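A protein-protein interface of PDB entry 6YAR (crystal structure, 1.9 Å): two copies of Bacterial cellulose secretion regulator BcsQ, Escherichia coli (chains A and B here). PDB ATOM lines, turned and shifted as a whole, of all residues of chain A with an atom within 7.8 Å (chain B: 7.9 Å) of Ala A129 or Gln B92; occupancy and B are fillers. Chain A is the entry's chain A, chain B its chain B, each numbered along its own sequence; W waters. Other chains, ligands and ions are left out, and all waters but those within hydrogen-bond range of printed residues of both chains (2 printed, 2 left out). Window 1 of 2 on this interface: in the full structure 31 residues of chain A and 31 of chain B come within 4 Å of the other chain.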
ATOM      1  N   GLN A   7      19.930   6.739  -2.596  1.00  0.00           N
ATOM      2  CA  GLN A   7      20.231   7.541  -3.782  1.00  0.00           C
ATOM      3  C   GLN A   7      20.197   6.652  -5.012  1.00  0.00           C
ATOM      4  O   GLN A   7      20.931   5.664  -5.078  1.00  0.00           O
ATOM      5  CB  GLN A   7      21.598   8.200  -3.652  1.00  0.00           C
ATOM      6  CG  GLN A   7      21.876   9.306  -4.685  1.00  0.00           C
ATOM      7  CD  GLN A   7      23.312   9.800  -4.612  1.00  0.00           C
ATOM      8  OE1 GLN A   7      24.243   9.003  -4.495  1.00  0.00           O
ATOM      9  NE2 GLN A   7      23.496  11.120  -4.688  1.00  0.00           N
ATOM     10  N   GLN A  99      21.812  26.713  -3.729  1.00  0.00           N
ATOM     11  CA  GLN A  99      22.411  25.444  -3.304  1.00  0.00           C
ATOM     12  C   GLN A  99      23.675  25.615  -2.467  1.00  0.00           C
ATOM     13  O   GLN A  99      24.243  24.607  -2.036  1.00  0.00           O
ATOM     14  CB  GLN A  99      22.700  24.549  -4.516  1.00  0.00           C
ATOM     15  CG  GLN A  99      23.761  25.072  -5.479  1.00  0.00           C
ATOM     16  CD  GLN A  99      23.808  24.280  -6.779  1.00  0.00           C
ATOM     17  OE1 GLN A  99      23.454  23.100  -6.813  1.00  0.00           O
ATOM     18  NE2 GLN A  99      24.232  24.931  -7.858  1.00  0.00           N
ATOM     19  N   PRO A 126      19.014  13.314  -4.009  1.00  0.00           N
ATOM     20  CA  PRO A 126      18.921  13.407  -5.466  1.00  0.00           C
ATOM     21  C   PRO A 126      20.193  12.896  -6.127  1.00  0.00           C
ATOM     22  O   PRO A 126      21.242  12.727  -5.492  1.00  0.00           O
ATOM     23  CB  PRO A 126      18.710  14.902  -5.716  1.00  0.00           C
ATOM     24  CG  PRO A 126      19.443  15.546  -4.597  1.00  0.00           C
ATOM     25  CD  PRO A 126      19.294  14.629  -3.398  1.00  0.00           C
ATOM     26  N   ARG A 127      20.050  12.605  -7.419  1.00  0.00           N
ATOM     27  CA  ARG A 127      21.147  12.167  -8.281  1.00  0.00           C
ATOM     28  C   ARG A 127      21.765  13.407  -8.925  1.00  0.00           C
ATOM     29  O   ARG A 127      21.633  13.679 -10.119  1.00  0.00           O
ATOM     30  CB  ARG A 127      20.645  11.169  -9.322  1.00  0.00           C
ATOM     31  CG  ARG A 127      21.694  10.670 -10.340  1.00  0.00           C
ATOM     32  CD  ARG A 127      22.579   9.573  -9.759  1.00  0.00           C
ATOM     33  NE  ARG A 127      23.951  10.003  -9.509  1.00  0.00           N
ATOM     34  CZ  ARG A 127      24.823   9.332  -8.757  1.00  0.00           C
ATOM     35  NH1 ARG A 127      24.472   8.198  -8.173  1.00  0.00           N
ATOM     36  NH2 ARG A 127      26.053   9.798  -8.584  1.00  0.00           N
ATOM     37  N   ASP A 128      22.402  14.203  -8.070  1.00  0.00           N
ATOM     38  CA  ASP A 128      23.202  15.326  -8.499  1.00  0.00           C
ATOM     39  C   ASP A 128      24.461  15.325  -7.650  1.00  0.00           C
ATOM     40  O   ASP A 128      24.595  14.558  -6.688  1.00  0.00           O
ATOM     41  CB  ASP A 128      22.442  16.667  -8.402  1.00  0.00           C
ATOM     42  CG  ASP A 128      22.063  17.062  -6.959  1.00  0.00           C
ATOM     43  OD1 ASP A 128      22.857  16.865  -6.012  1.00  0.00           O
ATOM     44  OD2 ASP A 128      20.964  17.628  -6.775  1.00  0.00           O
ATOM     45  N   ALA A 129      25.381  16.203  -8.003  1.00  0.00           N
ATOM     46  CA  ALA A 129      26.646  16.321  -7.304  1.00  0.00           C
ATOM     47  C   ALA A 129      26.763  17.662  -6.588  1.00  0.00           C
ATOM     48  O   ALA A 129      27.855  18.227  -6.499  1.00  0.00           O
ATOM     49  CB  ALA A 129      27.802  16.132  -8.284  1.00  0.00           C
ATOM     50  N   SER A 130      25.647  18.197  -6.091  1.00  0.00           N
ATOM     51  CA  SER A 130      25.714  19.507  -5.462  1.00  0.00           C
ATOM     52  C   SER A 130      26.435  19.406  -4.124  1.00  0.00           C
ATOM     53  O   SER A 130      26.670  18.316  -3.596  1.00  0.00           O
ATOM     54  CB  SER A 130      24.321  20.097  -5.261  1.00  0.00           C
ATOM     55  OG  SER A 130      23.589  19.341  -4.317  1.00  0.00           O
ATOM     56  N   GLN A 131      26.787  20.572  -3.575  1.00  0.00           N
ATOM     57  CA  GLN A 131      27.480  20.610  -2.292  1.00  0.00           C
ATOM     58  C   GLN A 131      26.603  20.037  -1.189  1.00  0.00           C
ATOM     59  O   GLN A 131      27.068  19.257  -0.349  1.00  0.00           O
ATOM     60  CB  GLN A 131      27.887  22.048  -1.954  1.00  0.00           C
ATOM     61  CG  GLN A 131      28.625  22.180  -0.614  1.00  0.00           C
ATOM     62  CD  GLN A 131      28.926  23.624  -0.210  1.00  0.00           C
ATOM     63  OE1 GLN A 131      28.141  24.540  -0.471  1.00  0.00           O
ATOM     64  NE2 GLN A 131      30.073  23.828   0.433  1.00  0.00           N
ATOM     65  N   ILE A 132      25.320  20.396  -1.198  1.00  0.00           N
ATOM     66  CA  ILE A 132      24.412  19.985  -0.141  1.00  0.00           C
ATOM     67  C   ILE A 132      24.135  18.483  -0.208  1.00  0.00           C
ATOM     68  O   ILE A 132      23.881  17.850   0.818  1.00  0.00           O
ATOM     69  CB  ILE A 132      23.125  20.828  -0.231  1.00  0.00           C
ATOM     70  CG1 ILE A 132      22.235  20.559   0.977  1.00  0.00           C
ATOM     71  CG2 ILE A 132      22.403  20.612  -1.585  1.00  0.00           C
ATOM     72  CD1 ILE A 132      22.933  20.908   2.268  1.00  0.00           C
ATOM     73  N   THR A 133      24.194  17.887  -1.404  1.00  0.00           N
ATOM     74  CA  THR A 133      24.044  16.436  -1.525  1.00  0.00           C
ATOM     75  C   THR A 133      25.264  15.718  -0.958  1.00  0.00           C
ATOM     76  O   THR A 133      25.135  14.728  -0.226  1.00  0.00           O
ATOM     77  CB  THR A 133      23.817  16.062  -2.994  1.00  0.00           C
ATOM     78  OG1 THR A 133      22.559  16.595  -3.420  1.00  0.00           O
ATOM     79  CG2 THR A 133      23.813  14.551  -3.201  1.00  0.00           C
ATOM     80  N   HIS A 134      26.460  16.208  -1.298  1.00  0.00           N
ATOM     81  CA  HIS A 134      27.697  15.630  -0.785  1.00  0.00           C
ATOM     82  C   HIS A 134      27.786  15.764   0.725  1.00  0.00           C
ATOM     83  O   HIS A 134      28.243  14.843   1.408  1.00  0.00           O
ATOM     84  CB  HIS A 134      28.905  16.310  -1.436  1.00  0.00           C
ATOM     85  CG  HIS A 134      29.102  15.939  -2.872  1.00  0.00           C
ATOM     86  ND1 HIS A 134      29.745  16.758  -3.774  1.00  0.00           N
ATOM     87  CD2 HIS A 134      28.732  14.834  -3.562  1.00  0.00           C
ATOM     88  CE1 HIS A 134      29.766  16.170  -4.958  1.00  0.00           C
ATOM     89  NE2 HIS A 134      29.158  15.001  -4.855  1.00  0.00           N
ATOM     90  N   ARG A 156      26.418   2.547 -15.933  1.00  0.00           N
ATOM     91  CA  ARG A 156      26.701   3.494 -14.861  1.00  0.00           C
ATOM     92  C   ARG A 156      27.529   2.857 -13.754  1.00  0.00           C
ATOM     93  O   ARG A 156      28.409   3.509 -13.177  1.00  0.00           O
ATOM     94  CB  ARG A 156      25.398   4.058 -14.303  1.00  0.00           C
ATOM     95  CG  ARG A 156      24.642   4.934 -15.302  1.00  0.00           C
ATOM     96  CD  ARG A 156      23.348   5.450 -14.691  1.00  0.00           C
ATOM     97  NE  ARG A 156      22.758   6.500 -15.516  1.00  0.00           N
ATOM     98  CZ  ARG A 156      23.024   7.793 -15.358  1.00  0.00           C
ATOM     99  NH1 ARG A 156      23.868   8.185 -14.397  1.00  0.00           N
ATOM    100  NH2 ARG A 156      22.459   8.688 -16.159  1.00  0.00           N
ATOM    101  N   HIS A 158      29.880   0.922 -14.074  1.00  0.00           N
ATOM    102  CA  HIS A 158      31.278   0.820 -14.472  1.00  0.00           C
ATOM    103  C   HIS A 158      31.946   2.175 -14.667  1.00  0.00           C
ATOM    104  O   HIS A 158      33.147   2.219 -14.942  1.00  0.00           O
ATOM    105  CB  HIS A 158      31.417  -0.012 -15.753  1.00  0.00           C
ATOM    106  CG  HIS A 158      31.077  -1.462 -15.575  1.00  0.00           C
ATOM    107  ND1 HIS A 158      29.779  -1.929 -15.571  1.00  0.00           N
ATOM    108  CD2 HIS A 158      31.865  -2.548 -15.394  1.00  0.00           C
ATOM    109  CE1 HIS A 158      29.782  -3.238 -15.397  1.00  0.00           C
ATOM    110  NE2 HIS A 158      31.035  -3.640 -15.282  1.00  0.00           N
ATOM    111  N   GLN A 159      31.214   3.279 -14.512  1.00  0.00           N
ATOM    112  CA  GLN A 159      31.795   4.581 -14.800  1.00  0.00           C
ATOM    113  C   GLN A 159      31.506   5.670 -13.776  1.00  0.00           C
ATOM    114  O   GLN A 159      32.142   6.727 -13.858  1.00  0.00           O
ATOM    115  CB  GLN A 159      31.326   5.076 -16.180  1.00  0.00           C
ATOM    116  CG  GLN A 159      29.860   5.481 -16.249  1.00  0.00           C
ATOM    117  CD  GLN A 159      29.508   6.095 -17.585  1.00  0.00           C
ATOM    118  OE1 GLN A 159      30.149   5.807 -18.598  1.00  0.00           O
ATOM    119  NE2 GLN A 159      28.497   6.961 -17.597  1.00  0.00           N
ATOM    120  N   GLN A 160      30.588   5.486 -12.832  1.00  0.00           N
ATOM    121  CA  GLN A 160      30.273   6.554 -11.899  1.00  0.00           C
ATOM    122  C   GLN A 160      30.495   6.084 -10.469  1.00  0.00           C
ATOM    123  O   GLN A 160      30.450   4.889 -10.174  1.00  0.00           O
ATOM    124  CB  GLN A 160      28.839   7.080 -12.083  1.00  0.00           C
ATOM    125  CG  GLN A 160      27.768   6.317 -11.393  1.00  0.00           C
ATOM    126  CD  GLN A 160      26.373   6.815 -11.767  1.00  0.00           C
ATOM    127  OE1 GLN A 160      26.094   7.108 -12.931  1.00  0.00           O
ATOM    128  NE2 GLN A 160      25.491   6.918 -10.771  1.00  0.00           N
ATOM    129  N   ALA A 161      30.789   7.036  -9.591  1.00  0.00           N
ATOM    130  CA  ALA A 161      31.028   6.705  -8.197  1.00  0.00           C
ATOM    131  C   ALA A 161      29.702   6.504  -7.480  1.00  0.00           C
ATOM    132  O   ALA A 161      28.700   7.160  -7.788  1.00  0.00           O
ATOM    133  CB  ALA A 161      31.843   7.797  -7.504  1.00  0.00           C
ATOM    134  N   LEU A 162      29.697   5.567  -6.568  1.00  0.00           N
ATOM    135  CA  LEU A 162      28.676   5.416  -5.558  1.00  0.00           C
ATOM    136  C   LEU A 162      29.209   5.927  -4.230  1.00  0.00           C
ATOM    137  O   LEU A 162      30.424   6.031  -4.038  1.00  0.00           O
ATOM    138  CB  LEU A 162      28.270   3.946  -5.426  1.00  0.00           C
ATOM    139  CG  LEU A 162      27.696   3.244  -6.655  1.00  0.00           C
ATOM    140  CD1 LEU A 162      27.037   1.961  -6.230  1.00  0.00           C
ATOM    141  CD2 LEU A 162      26.731   4.135  -7.439  1.00  0.00           C
ATOM    142  N   PRO B  40      26.418  14.849 -19.316  1.00  0.00           N
ATOM    143  CA  PRO B  40      27.746  14.445 -18.815  1.00  0.00           C
ATOM    144  C   PRO B  40      27.900  12.946 -18.647  1.00  0.00           C
ATOM    145  O   PRO B  40      29.039  12.465 -18.664  1.00  0.00           O
ATOM    146  CB  PRO B  40      27.855  15.172 -17.467  1.00  0.00           C
ATOM    147  CG  PRO B  40      26.970  16.368 -17.617  1.00  0.00           C
ATOM    148  CD  PRO B  40      25.831  15.950 -18.530  1.00  0.00           C
ATOM    149  N   ASP B  41      26.792  12.198 -18.496  1.00  0.00           N
ATOM    150  CA  ASP B  41      26.852  10.742 -18.422  1.00  0.00           C
ATOM    151  C   ASP B  41      27.453  10.117 -19.677  1.00  0.00           C
ATOM    152  O   ASP B  41      27.926   8.973 -19.619  1.00  0.00           O
ATOM    153  CB  ASP B  41      25.445  10.165 -18.212  1.00  0.00           C
ATOM    154  CG  ASP B  41      24.778  10.673 -16.950  1.00  0.00           C
ATOM    155  OD1 ASP B  41      25.355  10.488 -15.865  1.00  0.00           O
ATOM    156  OD2 ASP B  41      23.671  11.253 -17.040  1.00  0.00           O
ATOM    157  N   ARG B  55      37.334   8.013 -24.993  1.00  0.00           N
ATOM    158  CA  ARG B  55      36.976   9.052 -24.042  1.00  0.00           C
ATOM    159  C   ARG B  55      36.672  10.397 -24.694  1.00  0.00           C
ATOM    160  O   ARG B  55      36.100  11.265 -24.027  1.00  0.00           O
ATOM    161  CB  ARG B  55      38.093   9.204 -22.998  1.00  0.00           C
ATOM    162  CG  ARG B  55      38.200   8.001 -22.053  1.00  0.00           C
ATOM    163  CD  ARG B  55      39.329   8.164 -21.023  1.00  0.00           C
ATOM    164  NE  ARG B  55      39.165   9.355 -20.193  1.00  0.00           N
ATOM    165  CZ  ARG B  55      38.536   9.378 -19.019  1.00  0.00           C
ATOM    166  NH1 ARG B  55      38.001   8.267 -18.524  1.00  0.00           N
ATOM    167  NH2 ARG B  55      38.446  10.514 -18.335  1.00  0.00           N
ATOM    168  N   GLN B  86      34.185  11.417 -21.790  1.00  0.00           N
ATOM    169  CA  GLN B  86      34.215  10.793 -20.467  1.00  0.00           C
ATOM    170  C   GLN B  86      34.850  11.749 -19.457  1.00  0.00           C
ATOM    171  O   GLN B  86      35.999  12.177 -19.631  1.00  0.00           O
ATOM    172  CB  GLN B  86      34.986   9.468 -20.487  1.00  0.00           C
ATOM    173  CG  GLN B  86      34.247   8.267 -21.077  1.00  0.00           C
ATOM    174  CD  GLN B  86      32.946   7.932 -20.346  1.00  0.00           C
ATOM    175  OE1 GLN B  86      31.904   8.501 -20.639  1.00  0.00           O
ATOM    176  NE2 GLN B  86      33.010   6.997 -19.400  1.00  0.00           N
ATOM    177  N   LEU B  87      34.094  12.102 -18.425  1.00  0.00           N
ATOM    178  CA  LEU B  87      34.631  12.855 -17.298  1.00  0.00           C
ATOM    179  C   LEU B  87      35.233  11.894 -16.281  1.00  0.00           C
ATOM    180  O   LEU B  87      34.715  10.799 -16.067  1.00  0.00           O
ATOM    181  CB  LEU B  87      33.537  13.687 -16.626  1.00  0.00           C
ATOM    182  CG  LEU B  87      32.826  14.711 -17.508  1.00  0.00           C
ATOM    183  CD1 LEU B  87      31.693  15.356 -16.727  1.00  0.00           C
ATOM    184  CD2 LEU B  87      33.808  15.759 -18.034  1.00  0.00           C
ATOM    185  N   SER B  88      36.336  12.307 -15.659  1.00  0.00           N
ATOM    186  CA  SER B  88      36.876  11.552 -14.541  1.00  0.00           C
ATOM    187  C   SER B  88      35.902  11.586 -13.365  1.00  0.00           C
ATOM    188  O   SER B  88      34.978  12.403 -13.312  1.00  0.00           O
ATOM    189  CB  SER B  88      38.212  12.137 -14.103  1.00  0.00           C
ATOM    190  OG  SER B  88      37.957  13.359 -13.444  1.00  0.00           O
ATOM    191  N   ILE B  89      36.134  10.702 -12.391  1.00  0.00           N
ATOM    192  CA  ILE B  89      35.289  10.692 -11.197  1.00  0.00           C
ATOM    193  C   ILE B  89      35.312  12.060 -10.519  1.00  0.00           C
ATOM    194  O   ILE B  89      34.262  12.615 -10.166  1.00  0.00           O
ATOM    195  CB  ILE B  89      35.730   9.573 -10.237  1.00  0.00           C
ATOM    196  CG1 ILE B  89      35.408   8.200 -10.840  1.00  0.00           C
ATOM    197  CG2 ILE B  89      35.070   9.746  -8.867  1.00  0.00           C
ATOM    198  CD1 ILE B  89      33.939   7.998 -11.174  1.00  0.00           C
ATOM    199  N   GLU B  90      36.510  12.637 -10.362  1.00  0.00           N
ATOM    200  CA  GLU B  90      36.641  13.951  -9.735  1.00  0.00           C
ATOM    201  C   GLU B  90      35.858  15.016 -10.491  1.00  0.00           C
ATOM    202  O   GLU B  90      35.213  15.873  -9.872  1.00  0.00           O
ATOM    203  CB  GLU B  90      38.114  14.352  -9.641  1.00  0.00           C
ATOM    204  CG  GLU B  90      38.360  15.636  -8.839  1.00  0.00           C
ATOM    205  CD  GLU B  90      38.554  16.891  -9.709  1.00  0.00           C
ATOM    206  OE1 GLU B  90      38.811  16.763 -10.924  1.00  0.00           O
ATOM    207  OE2 GLU B  90      38.452  18.016  -9.168  1.00  0.00           O
ATOM    208  N   GLU B  91      35.921  14.999 -11.828  1.00  0.00           N
ATOM    209  CA  GLU B  91      35.139  15.960 -12.600  1.00  0.00           C
ATOM    210  C   GLU B  91      33.646  15.743 -12.405  1.00  0.00           C
ATOM    211  O   GLU B  91      32.895  16.710 -12.245  1.00  0.00           O
ATOM    212  CB  GLU B  91      35.504  15.882 -14.085  1.00  0.00           C
ATOM    213  CG  GLU B  91      36.909  16.399 -14.380  1.00  0.00           C
ATOM    214  CD  GLU B  91      37.335  16.115 -15.808  1.00  0.00           C
ATOM    215  OE1 GLU B  91      36.960  15.065 -16.360  1.00  0.00           O
ATOM    216  OE2 GLU B  91      38.037  16.948 -16.389  1.00  0.00           O
ATOM    217  N   GLN B  92      33.201  14.479 -12.408  1.00  0.00           N
ATOM    218  CA  GLN B  92      31.776  14.177 -12.231  1.00  0.00           C
ATOM    219  C   GLN B  92      31.244  14.724 -10.909  1.00  0.00           C
ATOM    220  O   GLN B  92      30.103  15.195 -10.836  1.00  0.00           O
ATOM    221  CB  GLN B  92      31.521  12.664 -12.287  1.00  0.00           C
ATOM    222  CG  GLN B  92      31.956  11.935 -13.550  1.00  0.00           C
ATOM    223  CD  GLN B  92      31.763  10.420 -13.437  1.00  0.00           C
ATOM    224  OE1 GLN B  92      30.815   9.963 -12.824  1.00  0.00           O
ATOM    225  NE2 GLN B  92      32.674   9.648 -14.019  1.00  0.00           N
ATOM    226  N   GLU B  93      32.041  14.655  -9.851  1.00  0.00           N
ATOM    227  CA  GLU B  93      31.565  15.086  -8.543  1.00  0.00           C
ATOM    228  C   GLU B  93      31.821  16.559  -8.271  1.00  0.00           C
ATOM    229  O   GLU B  93      31.508  17.034  -7.171  1.00  0.00           O
ATOM    230  CB  GLU B  93      32.196  14.228  -7.439  1.00  0.00           C
ATOM    231  CG  GLU B  93      31.739  12.757  -7.462  1.00  0.00           C
ATOM    232  CD  GLU B  93      30.220  12.599  -7.505  1.00  0.00           C
ATOM    233  OE1 GLU B  93      29.509  13.303  -6.758  1.00  0.00           O
ATOM    234  OE2 GLU B  93      29.730  11.770  -8.300  1.00  0.00           O
ATOM    235  N   ASN B  94      32.384  17.292  -9.229  1.00  0.00           N
ATOM    236  CA  ASN B  94      32.615  18.730  -9.087  1.00  0.00           C
ATOM    237  C   ASN B  94      32.174  19.453 -10.354  1.00  0.00           C
ATOM    238  O   ASN B  94      32.986  20.094 -11.033  1.00  0.00           O
ATOM    239  CB  ASN B  94      34.086  19.023  -8.791  1.00  0.00           C
ATOM    240  CG  ASN B  94      34.516  18.563  -7.421  1.00  0.00           C
ATOM    241  OD1 ASN B  94      34.349  19.279  -6.426  1.00  0.00           O
ATOM    242  ND2 ASN B  94      35.106  17.375  -7.360  1.00  0.00           N
ATOM    243  N   PRO B  95      30.878  19.401 -10.685  1.00  0.00           N
ATOM    244  CA  PRO B  95      30.419  20.066 -11.912  1.00  0.00           C
ATOM    245  C   PRO B  95      30.715  21.551 -11.932  1.00  0.00           C
ATOM    246  O   PRO B  95      30.863  22.121 -13.016  1.00  0.00           O
ATOM    247  CB  PRO B  95      28.909  19.785 -11.925  1.00  0.00           C
ATOM    248  CG  PRO B  95      28.568  19.500 -10.485  1.00  0.00           C
ATOM    249  CD  PRO B  95      29.762  18.805  -9.925  1.00  0.00           C
ATOM    250  N   GLN B  96      30.825  22.191 -10.765  1.00  0.00           N
ATOM    251  CA  GLN B  96      31.145  23.612 -10.714  1.00  0.00           C
ATOM    252  C   GLN B  96      32.538  23.907 -11.258  1.00  0.00           C
ATOM    253  O   GLN B  96      32.810  25.050 -11.630  1.00  0.00           O
ATOM    254  CB  GLN B  96      31.002  24.137  -9.278  1.00  0.00           C
ATOM    255  CG  GLN B  96      32.112  23.717  -8.291  1.00  0.00           C
ATOM    256  CD  GLN B  96      31.900  22.335  -7.661  1.00  0.00           C
ATOM    257  OE1 GLN B  96      31.050  21.549  -8.104  1.00  0.00           O
ATOM    258  NE2 GLN B  96      32.677  22.040  -6.613  1.00  0.00           N
ATOM    259  N   HIS B  97      33.417  22.904 -11.331  1.00  0.00           N
ATOM    260  CA  HIS B  97      34.751  23.115 -11.881  1.00  0.00           C
ATOM    261  C   HIS B  97      34.757  23.295 -13.402  1.00  0.00           C
ATOM    262  O   HIS B  97      35.727  23.838 -13.943  1.00  0.00           O
ATOM    263  CB  HIS B  97      35.666  21.946 -11.527  1.00  0.00           C
ATOM    264  CG  HIS B  97      36.004  21.850 -10.075  1.00  0.00           C
ATOM    265  ND1 HIS B  97      36.757  20.818  -9.563  1.00  0.00           N
ATOM    266  CD2 HIS B  97      35.706  22.658  -9.031  1.00  0.00           C
ATOM    267  CE1 HIS B  97      36.905  20.992  -8.261  1.00  0.00           C
ATOM    268  NE2 HIS B  97      36.282  22.103  -7.914  1.00  0.00           N
ATOM    269  N   TRP B  98      33.719  22.848 -14.112  1.00  0.00           N
ATOM    270  CA  TRP B  98      33.784  22.929 -15.568  1.00  0.00           C
ATOM    271  C   TRP B  98      32.503  23.384 -16.253  1.00  0.00           C
ATOM    272  O   TRP B  98      32.550  23.655 -17.459  1.00  0.00           O
ATOM    273  CB  TRP B  98      34.201  21.572 -16.145  1.00  0.00           C
ATOM    274  CG  TRP B  98      33.469  20.439 -15.528  1.00  0.00           C
ATOM    275  CD1 TRP B  98      33.894  19.662 -14.483  1.00  0.00           C
ATOM    276  CD2 TRP B  98      32.159  19.964 -15.876  1.00  0.00           C
ATOM    277  NE1 TRP B  98      32.936  18.731 -14.170  1.00  0.00           N
ATOM    278  CE2 TRP B  98      31.864  18.890 -15.015  1.00  0.00           C
ATOM    279  CE3 TRP B  98      31.212  20.341 -16.838  1.00  0.00           C
ATOM    280  CZ2 TRP B  98      30.651  18.187 -15.082  1.00  0.00           C
ATOM    281  CZ3 TRP B  98      30.011  19.642 -16.904  1.00  0.00           C
ATOM    282  CH2 TRP B  98      29.744  18.574 -16.038  1.00  0.00           C
HETATM  283  O   HOH W   1      27.463   7.811 -15.217  1.00  0.00           O
HETATM  284  O   HOH W   2      30.667   9.946 -10.162  1.00  0.00           O
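The side-chain amide nitrogen of Gln B92 lies within hydrogen-bond range of the backbone carbonyl oxygen of Gln A159, at 3.0 Å.
The side-chain amide nitrogen of Gln A159 sits at hydrogen-bond distance from the backbone carbonyl oxygen of Asp B41, at 2.9 Å.
The guanidinium group (NH2) of Arg A156 is in salt-bridge range of the side-chain carboxylate (OD2) of Asp B41, at 3.0 Å.
OE1 of Gln A159 lies within hydrogen-bond range of NE2 of Gln B86.
A ring nitrogen (NE2) of His A134 is in hydrogen-bond range of the side-chain carboxylate of Glu B93.
The guanidinium group (NH1) of Arg A127 sits close to the side-chain amide nitrogen (NE2) of Gln A160, at 3.1 Å.
The backbone carbonyl oxygen of Leu B87 sits at hydrogen-bond distance from the side-chain amide nitrogen of Gln B92 (3.1 Å).
A ring nitrogen (ND1) of His A134 lies within hydrogen-bond range of the backbone carbonyl oxygen (O) of Ser A130 (3.5 Å).
NH1 of Arg A156 lies within hydrogen-bond range of OE1 of Gln A160 (2.9 Å).
O of Arg B55 lies within hydrogen-bond range of N of Gln B86 (2.9 Å).
Among the printed residues, pairs that only touch across the chains: Gln A159 with Ile B89, Ala A129 with Gln B92, Gln A160 with Gln B92, Ala A129 with Glu B93, Ala A161 with Ile B89 and Ala A129 with Pro B95.
Of the printed residues of chain B, Ala A129 touches Gln B92 (3.6 Å), Glu B93 (3.6 Å) and Pro B95 (3.7 Å).
Of the printed residues of chain B, Arg A156 touches Asp B41 (3.0 Å).
Of the printed residues of chain B, Gln A159 touches Asp B41, Gln B86, Ile B89 and Gln B92.
Printed residues of chain B within 4 Å of Gln A160: Gln B92 (3.6 Å).
Printed residues of chain B within 4 Å of Ala A161: Ile B89.
Of chain A, only Ala A129 (3.6 Å), Gln A159 (3.0 Å) and Gln A160 (3.6 Å) come within 4 Å of Gln B92.
Printed residues of chain A within 4 Å of Pro B95: Ala A129.
Printed residues of chain A that touch a printed residue of chain B: Ala A129, His A134, Arg A156, Gln A159, Gln A160 and Ala A161.
Printed residues of chain B that touch a printed residue of chain A: Asp B41, Gln B86, Ile B89, Gln B92, Glu B93 and Pro B95.
Among the printed residues, Asp or Glu carboxylates within 4 Å of a Lys or Arg side-chain nitrogen of the other chain: Arg A156 with Asp B41.
No position is printed for both chains.
Water W2 lies within hydrogen-bond range of OE1 of Gln B92, OE2 of Glu B93 and N of Ala A161.
Water W1 lies within hydrogen-bond range of NE2 of Gln A159 (2.7 Å), OE1 of Gln A160 (2.8 Å) and OD1 of Asp B41 (3.5 Å).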
